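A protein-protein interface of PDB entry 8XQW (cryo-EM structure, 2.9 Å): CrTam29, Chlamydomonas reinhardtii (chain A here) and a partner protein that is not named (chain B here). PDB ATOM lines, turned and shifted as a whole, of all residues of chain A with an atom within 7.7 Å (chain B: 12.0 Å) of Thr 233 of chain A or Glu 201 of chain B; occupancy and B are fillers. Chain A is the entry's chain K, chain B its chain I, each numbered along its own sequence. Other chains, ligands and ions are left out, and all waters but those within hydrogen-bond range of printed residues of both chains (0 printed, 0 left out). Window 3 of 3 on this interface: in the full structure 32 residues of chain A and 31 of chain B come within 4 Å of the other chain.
The backbone carbonyl oxygen (O) of Glu 201 of chain B sits at hydrogen-bond distance from the guanidinium group (NH2) of Arg 235 of chain A, at 3.2 Å.
O of Leu 238 of chain A is in hydrogen-bond range of OH of Tyr 205 of chain B (2.6 Å).
The side-chain hydroxyl (OG1) of Thr 233 of chain A is in hydrogen-bond range of the guanidinium group (NE) of Arg 235 of chain A, at 2.6 Å.
The side-chain amide oxygen (OD1) of Asn 229 of chain A lies within hydrogen-bond range of the guanidinium group (NH2) of Arg 235 of chain A (3.1 Å).
Among the printed residues, pairs that only touch across the chains: Thr 233 of chain A with Trp 199 of chain B (3.5 Å), Asn 229 of chain A with Tyr 205 of chain B (3.6 Å), Asn 229 of chain A with Pro 204 of chain B (3.7 Å), Arg 235 of chain A with Pro 204 of chain B (3.7 Å) and Thr 233 of chain A with Glu 201 of chain B (3.9 Å).
Of chain B, only Trp 199 and Glu 201 come within 4 Å of Thr 233 of chain A.
Glu 201 of chain B touches just these residues of chain A: Thr 233 and Arg 235.
Gly 197 of chain A touches none of the printed residues of chain B.
Of chain B, only Pro 204 and Tyr 205 come within 4 Å of Asn 229 of chain A.
No residue of chain B comes within 4 Å of Lys 232 of chain A.
Gly 234 of chain A touches none of the printed residues of chain B.
Arg 235 of chain A touches just these residues of chain B: Glu 201 and Pro 204.
Printed residues of chain A within 4 Å of Tyr 205 of chain B: Asn 229 (3.6 Å) and Leu 238 (2.6 Å).
Printed residues of chain A within 4 Å of Pro 204 of chain B: Asn 229 and Arg 235.
Printed residues of chain B within 4 Å of Leu 238 of chain A: Tyr 205.
Trp 206 of chain B touches none of the printed residues of chain A.
Asp 203 of chain B touches none of the printed residues of chain A.
The nearest printed residue of chain A that does not touch Glu 201 of chain B is Asn 229 of chain A (5.9 Å).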
ATOM      1  N   LEU A 193     -17.374   0.786  12.562  1.00  0.00           N
ATOM      2  CA  LEU A 193     -16.158   0.471  13.306  1.00  0.00           C
ATOM      3  C   LEU A 193     -15.506  -0.814  12.816  1.00  0.00           C
ATOM      4  O   LEU A 193     -14.273  -0.929  12.813  1.00  0.00           O
ATOM      5  CB  LEU A 193     -16.486   0.355  14.788  1.00  0.00           C
ATOM      6  CG  LEU A 193     -15.517   0.932  15.796  1.00  0.00           C
ATOM      7  CD1 LEU A 193     -16.152   2.097  16.498  1.00  0.00           C
ATOM      8  CD2 LEU A 193     -15.197  -0.137  16.784  1.00  0.00           C
ATOM      9  N   ALA A 194     -16.315  -1.795  12.419  1.00  0.00           N
ATOM     10  CA  ALA A 194     -15.758  -3.028  11.880  1.00  0.00           C
ATOM     11  C   ALA A 194     -14.945  -2.782  10.623  1.00  0.00           C
ATOM     12  O   ALA A 194     -14.096  -3.606  10.274  1.00  0.00           O
ATOM     13  CB  ALA A 194     -16.867  -4.031  11.585  1.00  0.00           C
ATOM     14  N   ILE A 196     -12.813  -0.025  10.066  1.00  0.00           N
ATOM     15  CA  ILE A 196     -11.496   0.250  10.632  1.00  0.00           C
ATOM     16  C   ILE A 196     -10.846  -1.045  11.085  1.00  0.00           C
ATOM     17  O   ILE A 196      -9.696  -1.338  10.749  1.00  0.00           O
ATOM     18  CB  ILE A 196     -11.599   1.242  11.801  1.00  0.00           C
ATOM     19  CG1 ILE A 196     -11.883   2.650  11.301  1.00  0.00           C
ATOM     20  CG2 ILE A 196     -10.331   1.219  12.623  1.00  0.00           C
ATOM     21  CD1 ILE A 196     -13.328   3.028  11.404  1.00  0.00           C
ATOM     22  N   GLY A 197     -11.583  -1.838  11.854  1.00  0.00           N
ATOM     23  CA  GLY A 197     -11.065  -3.094  12.353  1.00  0.00           C
ATOM     24  C   GLY A 197     -10.474  -3.982  11.282  1.00  0.00           C
ATOM     25  O   GLY A 197      -9.278  -4.275  11.299  1.00  0.00           O
ATOM     26  N   SER A 198     -11.302  -4.412  10.332  1.00  0.00           N
ATOM     27  CA  SER A 198     -10.794  -5.247   9.255  1.00  0.00           C
ATOM     28  C   SER A 198      -9.916  -4.471   8.288  1.00  0.00           C
ATOM     29  O   SER A 198      -9.176  -5.082   7.512  1.00  0.00           O
ATOM     30  CB  SER A 198     -11.951  -5.884   8.493  1.00  0.00           C
ATOM     31  OG  SER A 198     -11.601  -6.077   7.136  1.00  0.00           O
ATOM     32  N   GLY A 199      -9.998  -3.144   8.299  1.00  0.00           N
ATOM     33  CA  GLY A 199      -9.190  -2.326   7.421  1.00  0.00           C
ATOM     34  C   GLY A 199      -9.686  -2.332   5.990  1.00  0.00           C
ATOM     35  O   GLY A 199      -9.471  -1.370   5.250  1.00  0.00           O
ATOM     36  N   THR A 202     -15.171  -5.527   5.219  1.00  0.00           N
ATOM     37  CA  THR A 202     -16.278  -5.729   6.152  1.00  0.00           C
ATOM     38  C   THR A 202     -17.033  -4.446   6.481  1.00  0.00           C
ATOM     39  O   THR A 202     -16.444  -3.458   6.931  1.00  0.00           O
ATOM     40  CB  THR A 202     -15.766  -6.368   7.442  1.00  0.00           C
ATOM     41  OG1 THR A 202     -14.674  -7.242   7.140  1.00  0.00           O
ATOM     42  CG2 THR A 202     -16.871  -7.168   8.104  1.00  0.00           C
ATOM     43  N   ALA A 227     -17.090  -3.855  21.387  1.00  0.00           N
ATOM     44  CA  ALA A 227     -16.572  -2.729  20.623  1.00  0.00           C
ATOM     45  C   ALA A 227     -15.080  -2.876  20.377  1.00  0.00           C
ATOM     46  O   ALA A 227     -14.599  -2.630  19.266  1.00  0.00           O
ATOM     47  CB  ALA A 227     -16.857  -1.425  21.352  1.00  0.00           C
ATOM     48  N   LEU A 228     -14.332  -3.279  21.404  1.00  0.00           N
ATOM     49  CA  LEU A 228     -12.891  -3.439  21.243  1.00  0.00           C
ATOM     50  C   LEU A 228     -12.562  -4.550  20.264  1.00  0.00           C
ATOM     51  O   LEU A 228     -11.671  -4.403  19.422  1.00  0.00           O
ATOM     52  CB  LEU A 228     -12.248  -3.724  22.588  1.00  0.00           C
ATOM     53  CG  LEU A 228     -10.826  -3.225  22.745  1.00  0.00           C
ATOM     54  CD1 LEU A 228     -10.859  -1.761  23.105  1.00  0.00           C
ATOM     55  CD2 LEU A 228     -10.107  -4.029  23.806  1.00  0.00           C
ATOM     56  N   ASN A 229     -13.254  -5.680  20.367  1.00  0.00           N
ATOM     57  CA  ASN A 229     -13.001  -6.779  19.448  1.00  0.00           C
ATOM     58  C   ASN A 229     -13.270  -6.356  18.015  1.00  0.00           C
ATOM     59  O   ASN A 229     -12.521  -6.710  17.099  1.00  0.00           O
ATOM     60  CB  ASN A 229     -13.859  -7.978  19.826  1.00  0.00           C
ATOM     61  CG  ASN A 229     -13.957  -8.985  18.724  1.00  0.00           C
ATOM     62  OD1 ASN A 229     -13.067  -9.803  18.543  1.00  0.00           O
ATOM     63  ND2 ASN A 229     -15.045  -8.940  17.978  1.00  0.00           N
ATOM     64  N   LEU A 230     -14.336  -5.586  17.803  1.00  0.00           N
ATOM     65  CA  LEU A 230     -14.628  -5.068  16.471  1.00  0.00           C
ATOM     66  C   LEU A 230     -13.513  -4.160  15.988  1.00  0.00           C
ATOM     67  O   LEU A 230     -12.989  -4.331  14.885  1.00  0.00           O
ATOM     68  CB  LEU A 230     -15.947  -4.307  16.479  1.00  0.00           C
ATOM     69  CG  LEU A 230     -17.247  -5.065  16.285  1.00  0.00           C
ATOM     70  CD1 LEU A 230     -18.363  -4.072  16.346  1.00  0.00           C
ATOM     71  CD2 LEU A 230     -17.261  -5.783  14.974  1.00  0.00           C
ATOM     72  N   TYR A 231     -13.141  -3.181  16.808  1.00  0.00           N
ATOM     73  CA  TYR A 231     -12.105  -2.232  16.432  1.00  0.00           C
ATOM     74  C   TYR A 231     -10.782  -2.902  16.117  1.00  0.00           C
ATOM     75  O   TYR A 231     -10.013  -2.370  15.314  1.00  0.00           O
ATOM     76  CB  TYR A 231     -11.899  -1.221  17.549  1.00  0.00           C
ATOM     77  CG  TYR A 231     -10.792  -0.240  17.296  1.00  0.00           C
ATOM     78  CD1 TYR A 231     -11.030   0.928  16.603  1.00  0.00           C
ATOM     79  CD2 TYR A 231      -9.515  -0.469  17.770  1.00  0.00           C
ATOM     80  CE1 TYR A 231     -10.029   1.835  16.375  1.00  0.00           C
ATOM     81  CE2 TYR A 231      -8.505   0.433  17.547  1.00  0.00           C
ATOM     82  CZ  TYR A 231      -8.769   1.583  16.849  1.00  0.00           C
ATOM     83  OH  TYR A 231      -7.767   2.493  16.621  1.00  0.00           O
ATOM     84  N   LYS A 232     -10.483  -4.039  16.735  1.00  0.00           N
ATOM     85  CA  LYS A 232      -9.157  -4.596  16.520  1.00  0.00           C
ATOM     86  C   LYS A 232      -9.123  -5.691  15.464  1.00  0.00           C
ATOM     87  O   LYS A 232      -8.177  -5.750  14.678  1.00  0.00           O
ATOM     88  CB  LYS A 232      -8.583  -5.113  17.835  1.00  0.00           C
ATOM     89  CG  LYS A 232      -8.479  -4.043  18.893  1.00  0.00           C
ATOM     90  CD  LYS A 232      -7.253  -4.241  19.750  1.00  0.00           C
ATOM     91  CE  LYS A 232      -6.865  -2.949  20.431  1.00  0.00           C
ATOM     92  NZ  LYS A 232      -7.143  -1.777  19.568  1.00  0.00           N
ATOM     93  N   THR A 233     -10.115  -6.579  15.423  1.00  0.00           N
ATOM     94  CA  THR A 233     -10.043  -7.697  14.493  1.00  0.00           C
ATOM     95  C   THR A 233     -11.263  -7.868  13.603  1.00  0.00           C
ATOM     96  O   THR A 233     -11.497  -8.982  13.126  1.00  0.00           O
ATOM     97  CB  THR A 233      -9.830  -9.019  15.240  1.00  0.00           C
ATOM     98  OG1 THR A 233     -11.099  -9.628  15.495  1.00  0.00           O
ATOM     99  CG2 THR A 233      -9.135  -8.785  16.554  1.00  0.00           C
ATOM    100  N   GLY A 234     -12.039  -6.818  13.354  1.00  0.00           N
ATOM    101  CA  GLY A 234     -13.263  -6.999  12.600  1.00  0.00           C
ATOM    102  C   GLY A 234     -14.155  -7.997  13.299  1.00  0.00           C
ATOM    103  O   GLY A 234     -14.719  -7.686  14.349  1.00  0.00           O
ATOM    104  N   ARG A 235     -14.276  -9.198  12.736  1.00  0.00           N
ATOM    105  CA  ARG A 235     -14.893 -10.349  13.399  1.00  0.00           C
ATOM    106  C   ARG A 235     -16.233  -9.978  14.023  1.00  0.00           C
ATOM    107  O   ARG A 235     -16.423 -10.014  15.236  1.00  0.00           O
ATOM    108  CB  ARG A 235     -13.952 -10.945  14.445  1.00  0.00           C
ATOM    109  CG  ARG A 235     -12.935 -11.893  13.869  1.00  0.00           C
ATOM    110  CD  ARG A 235     -12.356 -12.786  14.934  1.00  0.00           C
ATOM    111  NE  ARG A 235     -11.813 -12.024  16.050  1.00  0.00           N
ATOM    112  CZ  ARG A 235     -11.243 -12.574  17.111  1.00  0.00           C
ATOM    113  NH1 ARG A 235     -11.141 -13.889  17.198  1.00  0.00           N
ATOM    114  NH2 ARG A 235     -10.775 -11.813  18.086  1.00  0.00           N
ATOM    115  N   VAL A 236     -17.172  -9.609  13.156  1.00  0.00           N
ATOM    116  CA  VAL A 236     -18.424  -9.053  13.629  1.00  0.00           C
ATOM    117  C   VAL A 236     -19.316 -10.113  14.258  1.00  0.00           C
ATOM    118  O   VAL A 236     -20.284  -9.769  14.938  1.00  0.00           O
ATOM    119  CB  VAL A 236     -19.129  -8.336  12.463  1.00  0.00           C
ATOM    120  CG1 VAL A 236     -19.990  -9.293  11.695  1.00  0.00           C
ATOM    121  CG2 VAL A 236     -19.933  -7.170  12.958  1.00  0.00           C
ATOM    122  N   LEU A 238     -18.473 -12.527  16.526  1.00  0.00           N
ATOM    123  CA  LEU A 238     -18.029 -13.030  17.822  1.00  0.00           C
ATOM    124  C   LEU A 238     -18.721 -12.230  18.915  1.00  0.00           C
ATOM    125  O   LEU A 238     -18.409 -11.055  19.121  1.00  0.00           O
ATOM    126  CB  LEU A 238     -16.517 -12.921  17.943  1.00  0.00           C
ATOM    127  CG  LEU A 238     -15.741 -14.223  17.882  1.00  0.00           C
ATOM    128  CD1 LEU A 238     -14.356 -13.993  18.410  1.00  0.00           C
ATOM    129  CD2 LEU A 238     -16.442 -15.276  18.691  1.00  0.00           C
ATOM    130  N   TRP B 198      -6.142  -6.011  29.719  1.00  0.00           N
ATOM    131  CA  TRP B 198      -5.427  -5.995  28.453  1.00  0.00           C
ATOM    132  C   TRP B 198      -6.219  -6.718  27.372  1.00  0.00           C
ATOM    133  O   TRP B 198      -7.409  -6.970  27.527  1.00  0.00           O
ATOM    134  CB  TRP B 198      -4.043  -6.630  28.597  1.00  0.00           C
ATOM    135  CG  TRP B 198      -4.066  -8.079  28.949  1.00  0.00           C
ATOM    136  CD1 TRP B 198      -5.119  -8.789  29.425  1.00  0.00           C
ATOM    137  CD2 TRP B 198      -2.990  -9.010  28.806  1.00  0.00           C
ATOM    138  NE1 TRP B 198      -4.766 -10.099  29.612  1.00  0.00           N
ATOM    139  CE2 TRP B 198      -3.462 -10.261  29.236  1.00  0.00           C
ATOM    140  CE3 TRP B 198      -1.671  -8.905  28.364  1.00  0.00           C
ATOM    141  CZ2 TRP B 198      -2.665 -11.398  29.242  1.00  0.00           C
ATOM    142  CZ3 TRP B 198      -0.881 -10.035  28.368  1.00  0.00           C
ATOM    143  CH2 TRP B 198      -1.380 -11.266  28.804  1.00  0.00           C
ATOM    144  N   TRP B 199      -5.535  -7.069  26.288  1.00  0.00           N
ATOM    145  CA  TRP B 199      -6.158  -7.617  25.093  1.00  0.00           C
ATOM    146  C   TRP B 199      -5.670  -9.040  24.873  1.00  0.00           C
ATOM    147  O   TRP B 199      -4.485  -9.326  25.053  1.00  0.00           O
ATOM    148  CB  TRP B 199      -5.839  -6.740  23.882  1.00  0.00           C
ATOM    149  CG  TRP B 199      -6.128  -7.365  22.564  1.00  0.00           C
ATOM    150  CD1 TRP B 199      -5.222  -7.732  21.621  1.00  0.00           C
ATOM    151  CD2 TRP B 199      -7.413  -7.680  22.027  1.00  0.00           C
ATOM    152  NE1 TRP B 199      -5.859  -8.265  20.532  1.00  0.00           N
ATOM    153  CE2 TRP B 199      -7.208  -8.246  20.760  1.00  0.00           C
ATOM    154  CE3 TRP B 199      -8.719  -7.546  22.499  1.00  0.00           C
ATOM    155  CZ2 TRP B 199      -8.252  -8.676  19.960  1.00  0.00           C
ATOM    156  CZ3 TRP B 199      -9.753  -7.975  21.705  1.00  0.00           C
ATOM    157  CH2 TRP B 199      -9.515  -8.532  20.449  1.00  0.00           C
ATOM    158  N   ARG B 200      -6.586  -9.929  24.495  1.00  0.00           N
ATOM    159  CA  ARG B 200      -6.276 -11.338  24.249  1.00  0.00           C
ATOM    160  C   ARG B 200      -7.015 -11.759  22.986  1.00  0.00           C
ATOM    161  O   ARG B 200      -8.199 -12.094  23.039  1.00  0.00           O
ATOM    162  CB  ARG B 200      -6.664 -12.198  25.432  1.00  0.00           C
ATOM    163  CG  ARG B 200      -5.618 -12.265  26.511  1.00  0.00           C
ATOM    164  CD  ARG B 200      -5.995 -13.277  27.562  1.00  0.00           C
ATOM    165  NE  ARG B 200      -5.896 -12.708  28.895  1.00  0.00           N
ATOM    166  CZ  ARG B 200      -6.230 -13.352  30.002  1.00  0.00           C
ATOM    167  NH1 ARG B 200      -6.105 -12.755  31.174  1.00  0.00           N
ATOM    168  NH2 ARG B 200      -6.683 -14.593  29.935  1.00  0.00           N
ATOM    169  N   GLU B 201      -6.306 -11.769  21.858  1.00  0.00           N
ATOM    170  CA  GLU B 201      -6.957 -11.981  20.573  1.00  0.00           C
ATOM    171  C   GLU B 201      -7.608 -13.349  20.456  1.00  0.00           C
ATOM    172  O   GLU B 201      -8.573 -13.498  19.704  1.00  0.00           O
ATOM    173  CB  GLU B 201      -5.950 -11.798  19.444  1.00  0.00           C
ATOM    174  CG  GLU B 201      -6.541 -11.167  18.206  1.00  0.00           C
ATOM    175  CD  GLU B 201      -5.809 -11.565  16.945  1.00  0.00           C
ATOM    176  OE1 GLU B 201      -5.863 -12.756  16.578  1.00  0.00           O
ATOM    177  OE2 GLU B 201      -5.184 -10.686  16.317  1.00  0.00           O
ATOM    178  N   ASP B 202      -7.104 -14.349  21.170  1.00  0.00           N
ATOM    179  CA  ASP B 202      -7.652 -15.693  21.030  1.00  0.00           C
ATOM    180  C   ASP B 202      -9.059 -15.782  21.605  1.00  0.00           C
ATOM    181  O   ASP B 202      -9.969 -16.301  20.951  1.00  0.00           O
ATOM    182  CB  ASP B 202      -6.725 -16.702  21.696  1.00  0.00           C
ATOM    183  CG  ASP B 202      -5.284 -16.508  21.290  1.00  0.00           C
ATOM    184  OD1 ASP B 202      -4.697 -15.472  21.664  1.00  0.00           O
ATOM    185  OD2 ASP B 202      -4.738 -17.384  20.590  1.00  0.00           O
ATOM    186  N   ASP B 203      -9.256 -15.290  22.822  1.00  0.00           N
ATOM    187  CA  ASP B 203     -10.590 -15.114  23.391  1.00  0.00           C
ATOM    188  C   ASP B 203     -10.641 -13.727  24.005  1.00  0.00           C
ATOM    189  O   ASP B 203      -9.967 -13.475  25.024  1.00  0.00           O
ATOM    190  CB  ASP B 203     -10.924 -16.187  24.420  1.00  0.00           C
ATOM    191  CG  ASP B 203      -9.886 -16.294  25.499  1.00  0.00           C
ATOM    192  OD1 ASP B 203      -8.728 -15.924  25.235  1.00  0.00           O
ATOM    193  OD2 ASP B 203     -10.226 -16.744  26.612  1.00  0.00           O
ATOM    194  N   PRO B 204     -11.381 -12.810  23.435  1.00  0.00           N
ATOM    195  CA  PRO B 204     -11.351 -11.439  23.939  1.00  0.00           C
ATOM    196  C   PRO B 204     -12.187 -11.268  25.189  1.00  0.00           C
ATOM    197  O   PRO B 204     -11.901 -10.393  26.009  1.00  0.00           O
ATOM    198  CB  PRO B 204     -11.914 -10.625  22.770  1.00  0.00           C
ATOM    199  CG  PRO B 204     -11.987 -11.579  21.618  1.00  0.00           C
ATOM    200  CD  PRO B 204     -12.172 -12.914  22.206  1.00  0.00           C
ATOM    201  N   TYR B 205     -13.226 -12.081  25.344  1.00  0.00           N
ATOM    202  CA  TYR B 205     -14.135 -11.956  26.480  1.00  0.00           C
ATOM    203  C   TYR B 205     -13.762 -12.891  27.618  1.00  0.00           C
ATOM    204  O   TYR B 205     -14.584 -13.656  28.103  1.00  0.00           O
ATOM    205  CB  TYR B 205     -15.565 -12.205  26.030  1.00  0.00           C
ATOM    206  CG  TYR B 205     -15.861 -11.671  24.659  1.00  0.00           C
ATOM    207  CD1 TYR B 205     -15.903 -10.315  24.421  1.00  0.00           C
ATOM    208  CD2 TYR B 205     -16.097 -12.526  23.605  1.00  0.00           C
ATOM    209  CE1 TYR B 205     -16.163  -9.829  23.173  1.00  0.00           C
ATOM    210  CE2 TYR B 205     -16.363 -12.047  22.357  1.00  0.00           C
ATOM    211  CZ  TYR B 205     -16.395 -10.699  22.148  1.00  0.00           C
ATOM    212  OH  TYR B 205     -16.665 -10.221  20.894  1.00  0.00           O
ATOM    213  N   TRP B 206     -12.514 -12.838  28.052  1.00  0.00           N
ATOM    214  CA  TRP B 206     -12.105 -13.601  29.219  1.00  0.00           C
ATOM    215  C   TRP B 206     -12.629 -13.010  30.526  1.00  0.00           C
ATOM    216  O   TRP B 206     -12.883 -13.780  31.457  1.00  0.00           O
ATOM    217  CB  TRP B 206     -10.582 -13.742  29.269  1.00  0.00           C
ATOM    218  CG  TRP B 206      -9.850 -12.465  29.387  1.00  0.00           C
ATOM    219  CD1 TRP B 206      -9.398 -11.692  28.374  1.00  0.00           C
ATOM    220  CD2 TRP B 206      -9.474 -11.803  30.595  1.00  0.00           C
ATOM    221  NE1 TRP B 206      -8.768 -10.583  28.867  1.00  0.00           N
ATOM    222  CE2 TRP B 206      -8.802 -10.629  30.233  1.00  0.00           C
ATOM    223  CE3 TRP B 206      -9.649 -12.087  31.949  1.00  0.00           C
ATOM    224  CZ2 TRP B 206      -8.310  -9.738  31.172  1.00  0.00           C
ATOM    225  CZ3 TRP B 206      -9.160 -11.204  32.874  1.00  0.00           C
ATOM    226  CH2 TRP B 206      -8.497 -10.047  32.486  1.00  0.00           C
ATOM    227  N   PRO B 207     -12.806 -11.691  30.678  1.00  0.00           N
ATOM    228  CA  PRO B 207     -13.320 -11.202  31.963  1.00  0.00           C
ATOM    229  C   PRO B 207     -14.698 -11.723  32.317  1.00  0.00           C
ATOM    230  O   PRO B 207     -15.014 -11.826  33.504  1.00  0.00           O
ATOM    231  CB  PRO B 207     -13.328  -9.682  31.779  1.00  0.00           C
ATOM    232  CG  PRO B 207     -12.356  -9.425  30.763  1.00  0.00           C
ATOM    233  CD  PRO B 207     -12.465 -10.551  29.810  1.00  0.00           C
ATOM    234  N   ARG B 209     -16.013 -14.618  32.436  1.00  0.00           N
ATOM    235  CA  ARG B 209     -15.869 -16.059  32.505  1.00  0.00           C
ATOM    236  C   ARG B 209     -15.846 -16.460  33.965  1.00  0.00           C
ATOM    237  O   ARG B 209     -15.234 -15.788  34.792  1.00  0.00           O
ATOM    238  CB  ARG B 209     -14.597 -16.504  31.806  1.00  0.00           C
ATOM    239  CG  ARG B 209     -14.226 -17.936  32.029  1.00  0.00           C
ATOM    240  CD  ARG B 209     -14.503 -18.735  30.790  1.00  0.00           C
ATOM    241  NE  ARG B 209     -14.161 -17.985  29.590  1.00  0.00           N
ATOM    242  CZ  ARG B 209     -13.053 -18.177  28.887  1.00  0.00           C
ATOM    243  NH1 ARG B 209     -12.181 -19.099  29.266  1.00  0.00           N
ATOM    244  NH2 ARG B 209     -12.822 -17.451  27.804  1.00  0.00           N
